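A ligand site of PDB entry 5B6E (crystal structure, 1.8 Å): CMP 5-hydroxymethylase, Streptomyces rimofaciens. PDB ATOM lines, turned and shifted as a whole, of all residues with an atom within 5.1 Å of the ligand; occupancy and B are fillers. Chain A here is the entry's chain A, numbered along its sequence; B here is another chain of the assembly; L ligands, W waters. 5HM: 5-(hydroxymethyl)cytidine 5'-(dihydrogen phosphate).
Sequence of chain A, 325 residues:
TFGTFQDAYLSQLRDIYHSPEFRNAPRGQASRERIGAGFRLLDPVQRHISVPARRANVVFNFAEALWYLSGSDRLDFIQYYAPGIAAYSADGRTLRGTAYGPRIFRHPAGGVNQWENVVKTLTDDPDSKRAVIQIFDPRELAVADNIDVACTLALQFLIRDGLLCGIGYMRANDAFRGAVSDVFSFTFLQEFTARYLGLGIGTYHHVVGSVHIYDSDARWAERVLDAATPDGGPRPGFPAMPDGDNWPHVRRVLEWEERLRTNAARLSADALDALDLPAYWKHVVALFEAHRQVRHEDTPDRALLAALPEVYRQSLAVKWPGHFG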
ATOM      1  N   PRO A  26       7.683  33.637 -26.713  1.00  0.00           N
ATOM      2  CA  PRO A  26       8.509  32.434 -26.577  1.00  0.00           C
ATOM      3  C   PRO A  26       8.166  31.427 -27.668  1.00  0.00           C
ATOM      4  O   PRO A  26       6.988  31.148 -27.905  1.00  0.00           O
ATOM      5  CB  PRO A  26       8.133  31.884 -25.191  1.00  0.00           C
ATOM      6  CG  PRO A  26       7.449  33.006 -24.488  1.00  0.00           C
ATOM      7  CD  PRO A  26       6.798  33.838 -25.554  1.00  0.00           C
ATOM      8  N   ARG A  27       9.197  30.907 -28.339  1.00  0.00           N
ATOM      9  CA  ARG A  27       9.029  29.978 -29.454  1.00  0.00           C
ATOM     10  C   ARG A  27       8.045  30.521 -30.501  1.00  0.00           C
ATOM     11  O   ARG A  27       7.340  29.758 -31.174  1.00  0.00           O
ATOM     12  CB  ARG A  27       8.601  28.595 -28.936  1.00  0.00           C
ATOM     13  CG  ARG A  27       9.555  28.054 -27.868  1.00  0.00           C
ATOM     14  CD  ARG A  27       9.440  26.553 -27.648  1.00  0.00           C
ATOM     15  NE  ARG A  27       8.125  26.172 -27.115  1.00  0.00           N
ATOM     16  CZ  ARG A  27       7.228  25.406 -27.741  1.00  0.00           C
ATOM     17  NH1 ARG A  27       7.463  24.889 -28.952  1.00  0.00           N
ATOM     18  NH2 ARG A  27       6.071  25.141 -27.142  1.00  0.00           N
ATOM     19  N   TYR A  68      -2.977  10.282 -16.166  1.00  0.00           N
ATOM     20  CA  TYR A  68      -1.821  10.352 -15.255  1.00  0.00           C
ATOM     21  C   TYR A  68      -1.758   9.153 -14.315  1.00  0.00           C
ATOM     22  O   TYR A  68      -0.715   8.512 -14.191  1.00  0.00           O
ATOM     23  CB  TYR A  68      -1.829  11.640 -14.426  1.00  0.00           C
ATOM     24  CG  TYR A  68      -1.702  12.943 -15.194  1.00  0.00           C
ATOM     25  CD1 TYR A  68      -1.272  12.989 -16.518  1.00  0.00           C
ATOM     26  CD2 TYR A  68      -1.979  14.149 -14.552  1.00  0.00           C
ATOM     27  CE1 TYR A  68      -1.151  14.203 -17.188  1.00  0.00           C
ATOM     28  CE2 TYR A  68      -1.845  15.351 -15.207  1.00  0.00           C
ATOM     29  CZ  TYR A  68      -1.443  15.383 -16.526  1.00  0.00           C
ATOM     30  OH  TYR A  68      -1.335  16.599 -17.170  1.00  0.00           O
ATOM     31  N   TYR A  88       1.562  18.315 -29.774  1.00  0.00           N
ATOM     32  CA  TYR A  88       2.727  18.119 -28.910  1.00  0.00           C
ATOM     33  C   TYR A  88       3.346  16.726 -29.037  1.00  0.00           C
ATOM     34  O   TYR A  88       4.297  16.423 -28.329  1.00  0.00           O
ATOM     35  CB  TYR A  88       2.344  18.373 -27.451  1.00  0.00           C
ATOM     36  CG  TYR A  88       1.794  19.758 -27.239  1.00  0.00           C
ATOM     37  CD1 TYR A  88       2.641  20.834 -27.026  1.00  0.00           C
ATOM     38  CD2 TYR A  88       0.422  19.996 -27.287  1.00  0.00           C
ATOM     39  CE1 TYR A  88       2.134  22.117 -26.853  1.00  0.00           C
ATOM     40  CE2 TYR A  88      -0.092  21.272 -27.114  1.00  0.00           C
ATOM     41  CZ  TYR A  88       0.774  22.330 -26.889  1.00  0.00           C
ATOM     42  OH  TYR A  88       0.259  23.592 -26.719  1.00  0.00           O
ATOM     43  N   GLY A  97       6.894  15.489 -22.465  1.00  0.00           N
ATOM     44  CA  GLY A  97       6.709  16.389 -21.346  1.00  0.00           C
ATOM     45  C   GLY A  97       5.243  16.635 -20.944  1.00  0.00           C
ATOM     46  O   GLY A  97       4.969  17.070 -19.871  1.00  0.00           O
ATOM     47  N   THR A  98       4.317  16.378 -21.843  1.00  0.00           N
ATOM     48  CA  THR A  98       2.894  16.503 -21.528  1.00  0.00           C
ATOM     49  C   THR A  98       2.412  15.306 -20.679  1.00  0.00           C
ATOM     50  O   THR A  98       1.449  15.423 -19.915  1.00  0.00           O
ATOM     51  CB  THR A  98       2.059  16.643 -22.829  1.00  0.00           C
ATOM     52  OG1 THR A  98       2.371  17.895 -23.450  1.00  0.00           O
ATOM     53  CG2 THR A  98       0.558  16.590 -22.544  1.00  0.00           C
ATOM     54  N   TYR A 100       2.495  13.380 -17.733  1.00  0.00           N
ATOM     55  CA  TYR A 100       2.969  13.353 -16.348  1.00  0.00           C
ATOM     56  C   TYR A 100       2.884  11.959 -15.723  1.00  0.00           C
ATOM     57  O   TYR A 100       3.534  11.690 -14.731  1.00  0.00           O
ATOM     58  CB  TYR A 100       2.233  14.367 -15.484  1.00  0.00           C
ATOM     59  CG  TYR A 100       2.397  15.823 -15.891  1.00  0.00           C
ATOM     60  CD1 TYR A 100       3.492  16.255 -16.634  1.00  0.00           C
ATOM     61  CD2 TYR A 100       1.473  16.786 -15.488  1.00  0.00           C
ATOM     62  CE1 TYR A 100       3.654  17.589 -16.986  1.00  0.00           C
ATOM     63  CE2 TYR A 100       1.611  18.114 -15.844  1.00  0.00           C
ATOM     64  CZ  TYR A 100       2.698  18.512 -16.593  1.00  0.00           C
ATOM     65  OH  TYR A 100       2.848  19.830 -16.935  1.00  0.00           O
ATOM     66  N   ASP A 148       7.889  19.311 -26.869  1.00  0.00           N
ATOM     67  CA  ASP A 148       7.094  18.957 -25.683  1.00  0.00           C
ATOM     68  C   ASP A 148       7.953  18.792 -24.428  1.00  0.00           C
ATOM     69  O   ASP A 148       8.238  17.681 -23.996  1.00  0.00           O
ATOM     70  CB  ASP A 148       6.306  17.677 -25.965  1.00  0.00           C
ATOM     71  CG  ASP A 148       5.244  17.412 -24.922  1.00  0.00           C
ATOM     72  OD1 ASP A 148       4.731  18.385 -24.329  1.00  0.00           O
ATOM     73  OD2 ASP A 148       4.915  16.224 -24.697  1.00  0.00           O
ATOM     74  N   VAL A 149       8.327  19.924 -23.841  1.00  0.00           N
ATOM     75  CA  VAL A 149       9.152  19.960 -22.633  1.00  0.00           C
ATOM     76  C   VAL A 149       8.246  20.172 -21.422  1.00  0.00           C
ATOM     77  O   VAL A 149       7.439  21.094 -21.419  1.00  0.00           O
ATOM     78  CB  VAL A 149      10.166  21.121 -22.718  1.00  0.00           C
ATOM     79  CG1 VAL A 149      10.948  21.291 -21.421  1.00  0.00           C
ATOM     80  CG2 VAL A 149      11.104  20.907 -23.897  1.00  0.00           C
ATOM     81  N   CYS A 151       6.340  21.378 -18.379  1.00  0.00           N
ATOM     82  CA  CYS A 151       6.276  22.722 -17.778  1.00  0.00           C
ATOM     83  C   CYS A 151       5.987  22.687 -16.280  1.00  0.00           C
ATOM     84  O   CYS A 151       6.050  23.710 -15.604  1.00  0.00           O
ATOM     85  CB  CYS A 151       5.282  23.619 -18.530  1.00  0.00           C
ATOM     86  SG  CYS A 151       3.563  23.079 -18.451  1.00  0.00           S
ATOM     87  N   MET A 170       5.457  25.072 -11.118  1.00  0.00           N
ATOM     88  CA  MET A 170       5.552  25.063 -12.578  1.00  0.00           C
ATOM     89  C   MET A 170       6.489  26.150 -13.078  1.00  0.00           C
ATOM     90  O   MET A 170       6.504  27.242 -12.531  1.00  0.00           O
ATOM     91  CB  MET A 170       4.169  25.265 -13.212  1.00  0.00           C
ATOM     92  CG  MET A 170       3.096  24.298 -12.738  1.00  0.00           C
ATOM     93  SD  MET A 170       1.515  24.516 -13.588  1.00  0.00           S
ATOM     94  CE  MET A 170       1.927  23.828 -15.185  1.00  0.00           C
ATOM     95  N   ARG A 171       7.263  25.853 -14.119  1.00  0.00           N
ATOM     96  CA  ARG A 171       8.112  26.864 -14.771  1.00  0.00           C
ATOM     97  C   ARG A 171       7.267  27.788 -15.638  1.00  0.00           C
ATOM     98  O   ARG A 171       7.655  28.929 -15.892  1.00  0.00           O
ATOM     99  CB  ARG A 171       9.217  26.219 -15.603  1.00  0.00           C
ATOM    100  CG  ARG A 171       8.723  25.399 -16.785  1.00  0.00           C
ATOM    101  CD  ARG A 171       9.844  24.919 -17.698  1.00  0.00           C
ATOM    102  NE  ARG A 171       9.272  24.140 -18.792  1.00  0.00           N
ATOM    103  CZ  ARG A 171       8.691  24.646 -19.875  1.00  0.00           C
ATOM    104  NH1 ARG A 171       8.612  25.974 -20.069  1.00  0.00           N
ATOM    105  NH2 ARG A 171       8.177  23.834 -20.780  1.00  0.00           N
ATOM    106  N   ALA A 172       6.120  27.295 -16.109  1.00  0.00           N
ATOM    107  CA  ALA A 172       5.278  28.029 -17.034  1.00  0.00           C
ATOM    108  C   ALA A 172       3.870  27.474 -16.978  1.00  0.00           C
ATOM    109  O   ALA A 172       3.677  26.278 -16.744  1.00  0.00           O
ATOM    110  CB  ALA A 172       5.824  27.911 -18.455  1.00  0.00           C
ATOM    111  N   ASN A 173       2.866  28.328 -17.147  1.00  0.00           N
ATOM    112  CA  ASN A 173       1.480  27.875 -17.159  1.00  0.00           C
ATOM    113  C   ASN A 173       0.600  28.823 -17.965  1.00  0.00           C
ATOM    114  O   ASN A 173       0.626  30.026 -17.770  1.00  0.00           O
ATOM    115  CB  ASN A 173       0.960  27.741 -15.722  1.00  0.00           C
ATOM    116  CG  ASN A 173      -0.271  26.842 -15.601  1.00  0.00           C
ATOM    117  OD1 ASN A 173      -0.535  25.967 -16.437  1.00  0.00           O
ATOM    118  ND2 ASN A 173      -1.031  27.055 -14.542  1.00  0.00           N
ATOM    119  N   ASP A 174      -0.133  28.243 -18.917  1.00  0.00           N
ATOM    120  CA  ASP A 174      -1.161  28.930 -19.700  1.00  0.00           C
ATOM    121  C   ASP A 174      -2.334  29.251 -18.779  1.00  0.00           C
ATOM    122  O   ASP A 174      -3.061  28.362 -18.326  1.00  0.00           O
ATOM    123  CB  ASP A 174      -1.570  27.986 -20.832  1.00  0.00           C
ATOM    124  CG  ASP A 174      -2.688  28.532 -21.709  1.00  0.00           C
ATOM    125  OD1 ASP A 174      -3.322  29.553 -21.390  1.00  0.00           O
ATOM    126  OD2 ASP A 174      -2.924  27.886 -22.754  1.00  0.00           O
ATOM    127  N   GLY A 178      -4.420  25.800 -20.043  1.00  0.00           N
ATOM    128  CA  GLY A 178      -3.697  24.780 -19.271  1.00  0.00           C
ATOM    129  C   GLY A 178      -3.980  24.796 -17.772  1.00  0.00           C
ATOM    130  O   GLY A 178      -4.148  23.737 -17.168  1.00  0.00           O
ATOM    131  N   ALA A 179      -4.024  25.992 -17.192  1.00  0.00           N
ATOM    132  CA  ALA A 179      -4.280  26.146 -15.764  1.00  0.00           C
ATOM    133  C   ALA A 179      -5.550  25.418 -15.310  1.00  0.00           C
ATOM    134  O   ALA A 179      -5.597  24.876 -14.206  1.00  0.00           O
ATOM    135  CB  ALA A 179      -4.352  27.614 -15.377  1.00  0.00           C
ATOM    136  N   ASP A 182      -4.588  21.676 -15.343  1.00  0.00           N
ATOM    137  CA  ASP A 182      -3.466  21.412 -14.429  1.00  0.00           C
ATOM    138  C   ASP A 182      -3.912  21.474 -12.977  1.00  0.00           C
ATOM    139  O   ASP A 182      -3.611  20.565 -12.198  1.00  0.00           O
ATOM    140  CB  ASP A 182      -2.302  22.385 -14.671  1.00  0.00           C
ATOM    141  CG  ASP A 182      -1.644  22.187 -16.018  1.00  0.00           C
ATOM    142  OD1 ASP A 182      -1.636  21.044 -16.541  1.00  0.00           O
ATOM    143  OD2 ASP A 182      -1.121  23.175 -16.577  1.00  0.00           O
ATOM    144  N   HIS A 212       0.849  33.253 -18.390  1.00  0.00           N
ATOM    145  CA  HIS A 212       0.617  33.982 -19.621  1.00  0.00           C
ATOM    146  C   HIS A 212      -0.718  33.639 -20.265  1.00  0.00           C
ATOM    147  O   HIS A 212      -1.227  32.572 -20.085  1.00  0.00           O
ATOM    148  CB  HIS A 212       1.729  33.676 -20.595  1.00  0.00           C
ATOM    149  CG  HIS A 212       2.098  32.228 -20.628  1.00  0.00           C
ATOM    150  ND1 HIS A 212       3.105  31.701 -19.874  1.00  0.00           N
ATOM    151  CD2 HIS A 212       1.545  31.186 -21.288  1.00  0.00           C
ATOM    152  CE1 HIS A 212       3.164  30.399 -20.065  1.00  0.00           C
ATOM    153  NE2 HIS A 212       2.218  30.065 -20.913  1.00  0.00           N
ATOM    154  N   TYR A 214      -1.925  33.476 -24.194  1.00  0.00           N
ATOM    155  CA  TYR A 214      -1.513  33.563 -25.598  1.00  0.00           C
ATOM    156  C   TYR A 214      -2.431  34.526 -26.336  1.00  0.00           C
ATOM    157  O   TYR A 214      -3.639  34.531 -26.105  1.00  0.00           O
ATOM    158  CB  TYR A 214      -1.549  32.187 -26.263  1.00  0.00           C
ATOM    159  CG  TYR A 214      -0.526  31.238 -25.694  1.00  0.00           C
ATOM    160  CD1 TYR A 214       0.830  31.408 -25.958  1.00  0.00           C
ATOM    161  CD2 TYR A 214      -0.910  30.167 -24.876  1.00  0.00           C
ATOM    162  CE1 TYR A 214       1.778  30.545 -25.431  1.00  0.00           C
ATOM    163  CE2 TYR A 214       0.031  29.297 -24.348  1.00  0.00           C
ATOM    164  CZ  TYR A 214       1.373  29.495 -24.634  1.00  0.00           C
ATOM    165  OH  TYR A 214       2.321  28.631 -24.106  1.00  0.00           O
ATOM    166  N   LYS B 129      10.673  30.179 -21.909  1.00  0.00           N
ATOM    167  CA  LYS B 129      10.174  29.835 -20.574  1.00  0.00           C
ATOM    168  C   LYS B 129      10.769  28.516 -20.084  1.00  0.00           C
ATOM    169  O   LYS B 129      10.425  28.030 -19.004  1.00  0.00           O
ATOM    170  CB  LYS B 129       8.638  29.700 -20.611  1.00  0.00           C
ATOM    171  CG  LYS B 129       7.908  30.958 -21.064  1.00  0.00           C
ATOM    172  CD  LYS B 129       6.436  30.701 -21.366  1.00  0.00           C
ATOM    173  CE  LYS B 129       6.248  29.896 -22.637  1.00  0.00           C
ATOM    174  NZ  LYS B 129       4.841  29.807 -23.079  1.00  0.00           N
ATOM    175  N   ARG B 130      11.679  27.942 -20.871  1.00  0.00           N
ATOM    176  CA  ARG B 130      12.192  26.591 -20.633  1.00  0.00           C
ATOM    177  C   ARG B 130      13.555  26.540 -19.955  1.00  0.00           C
ATOM    178  O   ARG B 130      14.072  25.441 -19.709  1.00  0.00           O
ATOM    179  CB  ARG B 130      12.326  25.843 -21.956  1.00  0.00           C
ATOM    180  CG  ARG B 130      11.025  25.520 -22.660  1.00  0.00           C
ATOM    181  CD  ARG B 130      11.335  24.974 -24.041  1.00  0.00           C
ATOM    182  NE  ARG B 130      10.193  24.312 -24.663  1.00  0.00           N
ATOM    183  CZ  ARG B 130      10.265  23.609 -25.795  1.00  0.00           C
ATOM    184  NH1 ARG B 130      11.422  23.461 -26.432  1.00  0.00           N
ATOM    185  NH2 ARG B 130       9.175  23.043 -26.280  1.00  0.00           N
HETATM  186  OP3 5HM L   1       7.571  26.937 -24.455  1.00  0.00           O
HETATM  187  P   5HM L   1       6.980  25.984 -23.480  1.00  0.00           P
HETATM  188  OP1 5HM L   1       6.827  26.659 -22.029  1.00  0.00           O
HETATM  189  OP2 5HM L   1       7.846  24.642 -23.347  1.00  0.00           O
HETATM  190  O5' 5HM L   1       5.529  25.631 -24.092  1.00  0.00           O
HETATM  191  C5' 5HM L   1       4.630  24.758 -23.400  1.00  0.00           C
HETATM  192  C4' 5HM L   1       3.462  25.602 -22.909  1.00  0.00           C
HETATM  193  O4' 5HM L   1       2.273  24.811 -22.882  1.00  0.00           O
HETATM  194  C3' 5HM L   1       3.622  26.159 -21.508  1.00  0.00           C
HETATM  195  O3' 5HM L   1       4.370  27.382 -21.464  1.00  0.00           O
HETATM  196  C2' 5HM L   1       2.176  26.341 -21.117  1.00  0.00           C
HETATM  197  O2' 5HM L   1       1.659  27.533 -21.727  1.00  0.00           O
HETATM  198  C1' 5HM L   1       1.425  25.200 -21.784  1.00  0.00           C
HETATM  199  N1  5HM L   1       1.128  24.031 -20.931  1.00  0.00           N
HETATM  200  C2  5HM L   1       0.449  24.159 -19.682  1.00  0.00           C
HETATM  201  O2  5HM L   1       0.130  25.283 -19.240  1.00  0.00           O
HETATM  202  C6  5HM L   1       1.440  22.813 -21.405  1.00  0.00           C
HETATM  203  C5  5HM L   1       1.165  21.656 -20.674  1.00  0.00           C
HETATM  204  CM5 5HM L   1       1.576  20.318 -21.272  1.00  0.00           C
HETATM  205  OM5 5HM L   1       1.038  20.187 -22.591  1.00  0.00           O
HETATM  206  C4  5HM L   1       0.479  21.809 -19.373  1.00  0.00           C
HETATM  207  N3  5HM L   1       0.167  23.052 -18.946  1.00  0.00           N
HETATM  208  N4  5HM L   1       0.173  20.729 -18.591  1.00  0.00           N
HETATM  209  O   HOH W   1       5.621  28.699 -25.560  1.00  0.00           O
HETATM  210  O   HOH W   2       9.631  28.736 -24.046  1.00  0.00           O
HETATM  211  O   HOH W   3       4.766  21.554 -21.552  1.00  0.00           O
HETATM  212  O   HOH W   4       6.945  22.326 -24.616  1.00  0.00           O
HETATM  213  O   HOH W   5       4.055  19.787 -19.324  1.00  0.00           O
HETATM  214  O   HOH W   6       0.004  17.722 -19.159  1.00  0.00           O
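The backbone NH (N) of Asp 174 sits at hydrogen-bond distance from an oxygen (O2) of the ligand. An oxygen (OP2) of the ligand is in salt-bridge range of the guanidinium group (NH2) of Arg 171 (2.7 Å). The side-chain amide oxygen of Asn 173 lies close to an oxygen (O2) of the ligand. NE of Arg 27 lies within salt-bridge range of OP3 of the ligand (2.8 Å). NE of Arg 130 of chain B is in salt-bridge range of OP2 of the ligand (2.7 Å). O2' of the ligand lies within hydrogen-bond range of OH of Tyr 214, 2.7 Å away. OP1 of the ligand lies within salt-bridge range of NZ of Lys 129 of chain B (3.9 Å). N3 of the ligand lies within hydrogen-bond range of OD2 of Asp 182, at 2.7 Å. N3 of the ligand sits at hydrogen-bond distance from SG of Cys 151 (3.4 Å). The side-chain hydroxyl (OG1) of Thr 98 lies within hydrogen-bond range of an oxygen (OM5) of the ligand. A ring nitrogen (NE2) of His 212 lies within hydrogen-bond range of an oxygen (O2') of the ligand (2.7 Å). A nitrogen (N4) of the ligand is in hydrogen-bond range of the side-chain hydroxyl (OH) of Tyr 100.
Ala 172 touches the ligand. Gly 178 touches the ligand (CA to O2, 3.9 Å). Hydrophobic or aromatic side chains that line the ligand: Tyr 100, Ala 172, His 212 and Tyr 214. Of the 22 residues printed, 14 come within 4 Å of the ligand. Along chain A the residues within 4 Å of the ligand span positions 27 to 214.
Water W2 lies within hydrogen-bond range of an oxygen (OP3) of the ligand and the backbone NH of Lys 129 of chain B. Water W4 lies within hydrogen-bond range of an oxygen (OP2) of the ligand (2.8 Å), the guanidinium group of Arg 130 of chain B (2.9 Å) and the backbone NH of Val 149 (2.9 Å). Water W1 lies within hydrogen-bond range of the side-chain amino group of Lys 129 of chain B (2.8 Å) and an oxygen (OP3) of the ligand (2.9 Å). Water W6 lies within hydrogen-bond range of OH of Tyr 68 (2.6 Å), O of Thr 98 (2.8 Å) and N4 of the ligand (3.1 Å). Water W5 lies within hydrogen-bond range of OH of Tyr 100 (2.7 Å), O of Gly 97 (2.9 Å) and N of Cys 151 (2.9 Å). Water W3 lies within hydrogen-bond range of the backbone carbonyl oxygen (O) of Val 149 (2.7 Å) and the side-chain sulfur (SG) of Cys 151 (3.7 Å).
The guanidinium group (NH1) of Arg 171 is in hydrogen-bond range of the backbone carbonyl oxygen (O) of Lys 129 of chain B. NH2 of Arg 171 is in hydrogen-bond range of O of Val 149, at 2.9 Å. OH of Tyr 100 lies within hydrogen-bond range of SG of Cys 151, 3.7 Å away. The side-chain amide nitrogen (ND2) of Asn 173 sits close to the side-chain sulfur (SD) of Met 170, at 3.7 Å. The backbone carbonyl oxygen (O) of Ala 172 lies close to the side-chain sulfur (SG) of Cys 151 (3.6 Å). The side-chain hydroxyl (OG1) of Thr 98 sits at hydrogen-bond distance from the side-chain carboxylate (OD1) of Asp 148. NE2 of His 212 lies within hydrogen-bond range of NZ of Lys 129 of chain B, 3.4 Å away. The backbone carbonyl oxygen (O) of Cys 151 lies within hydrogen-bond range of the backbone NH (N) of Arg 171 (2.9 Å).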
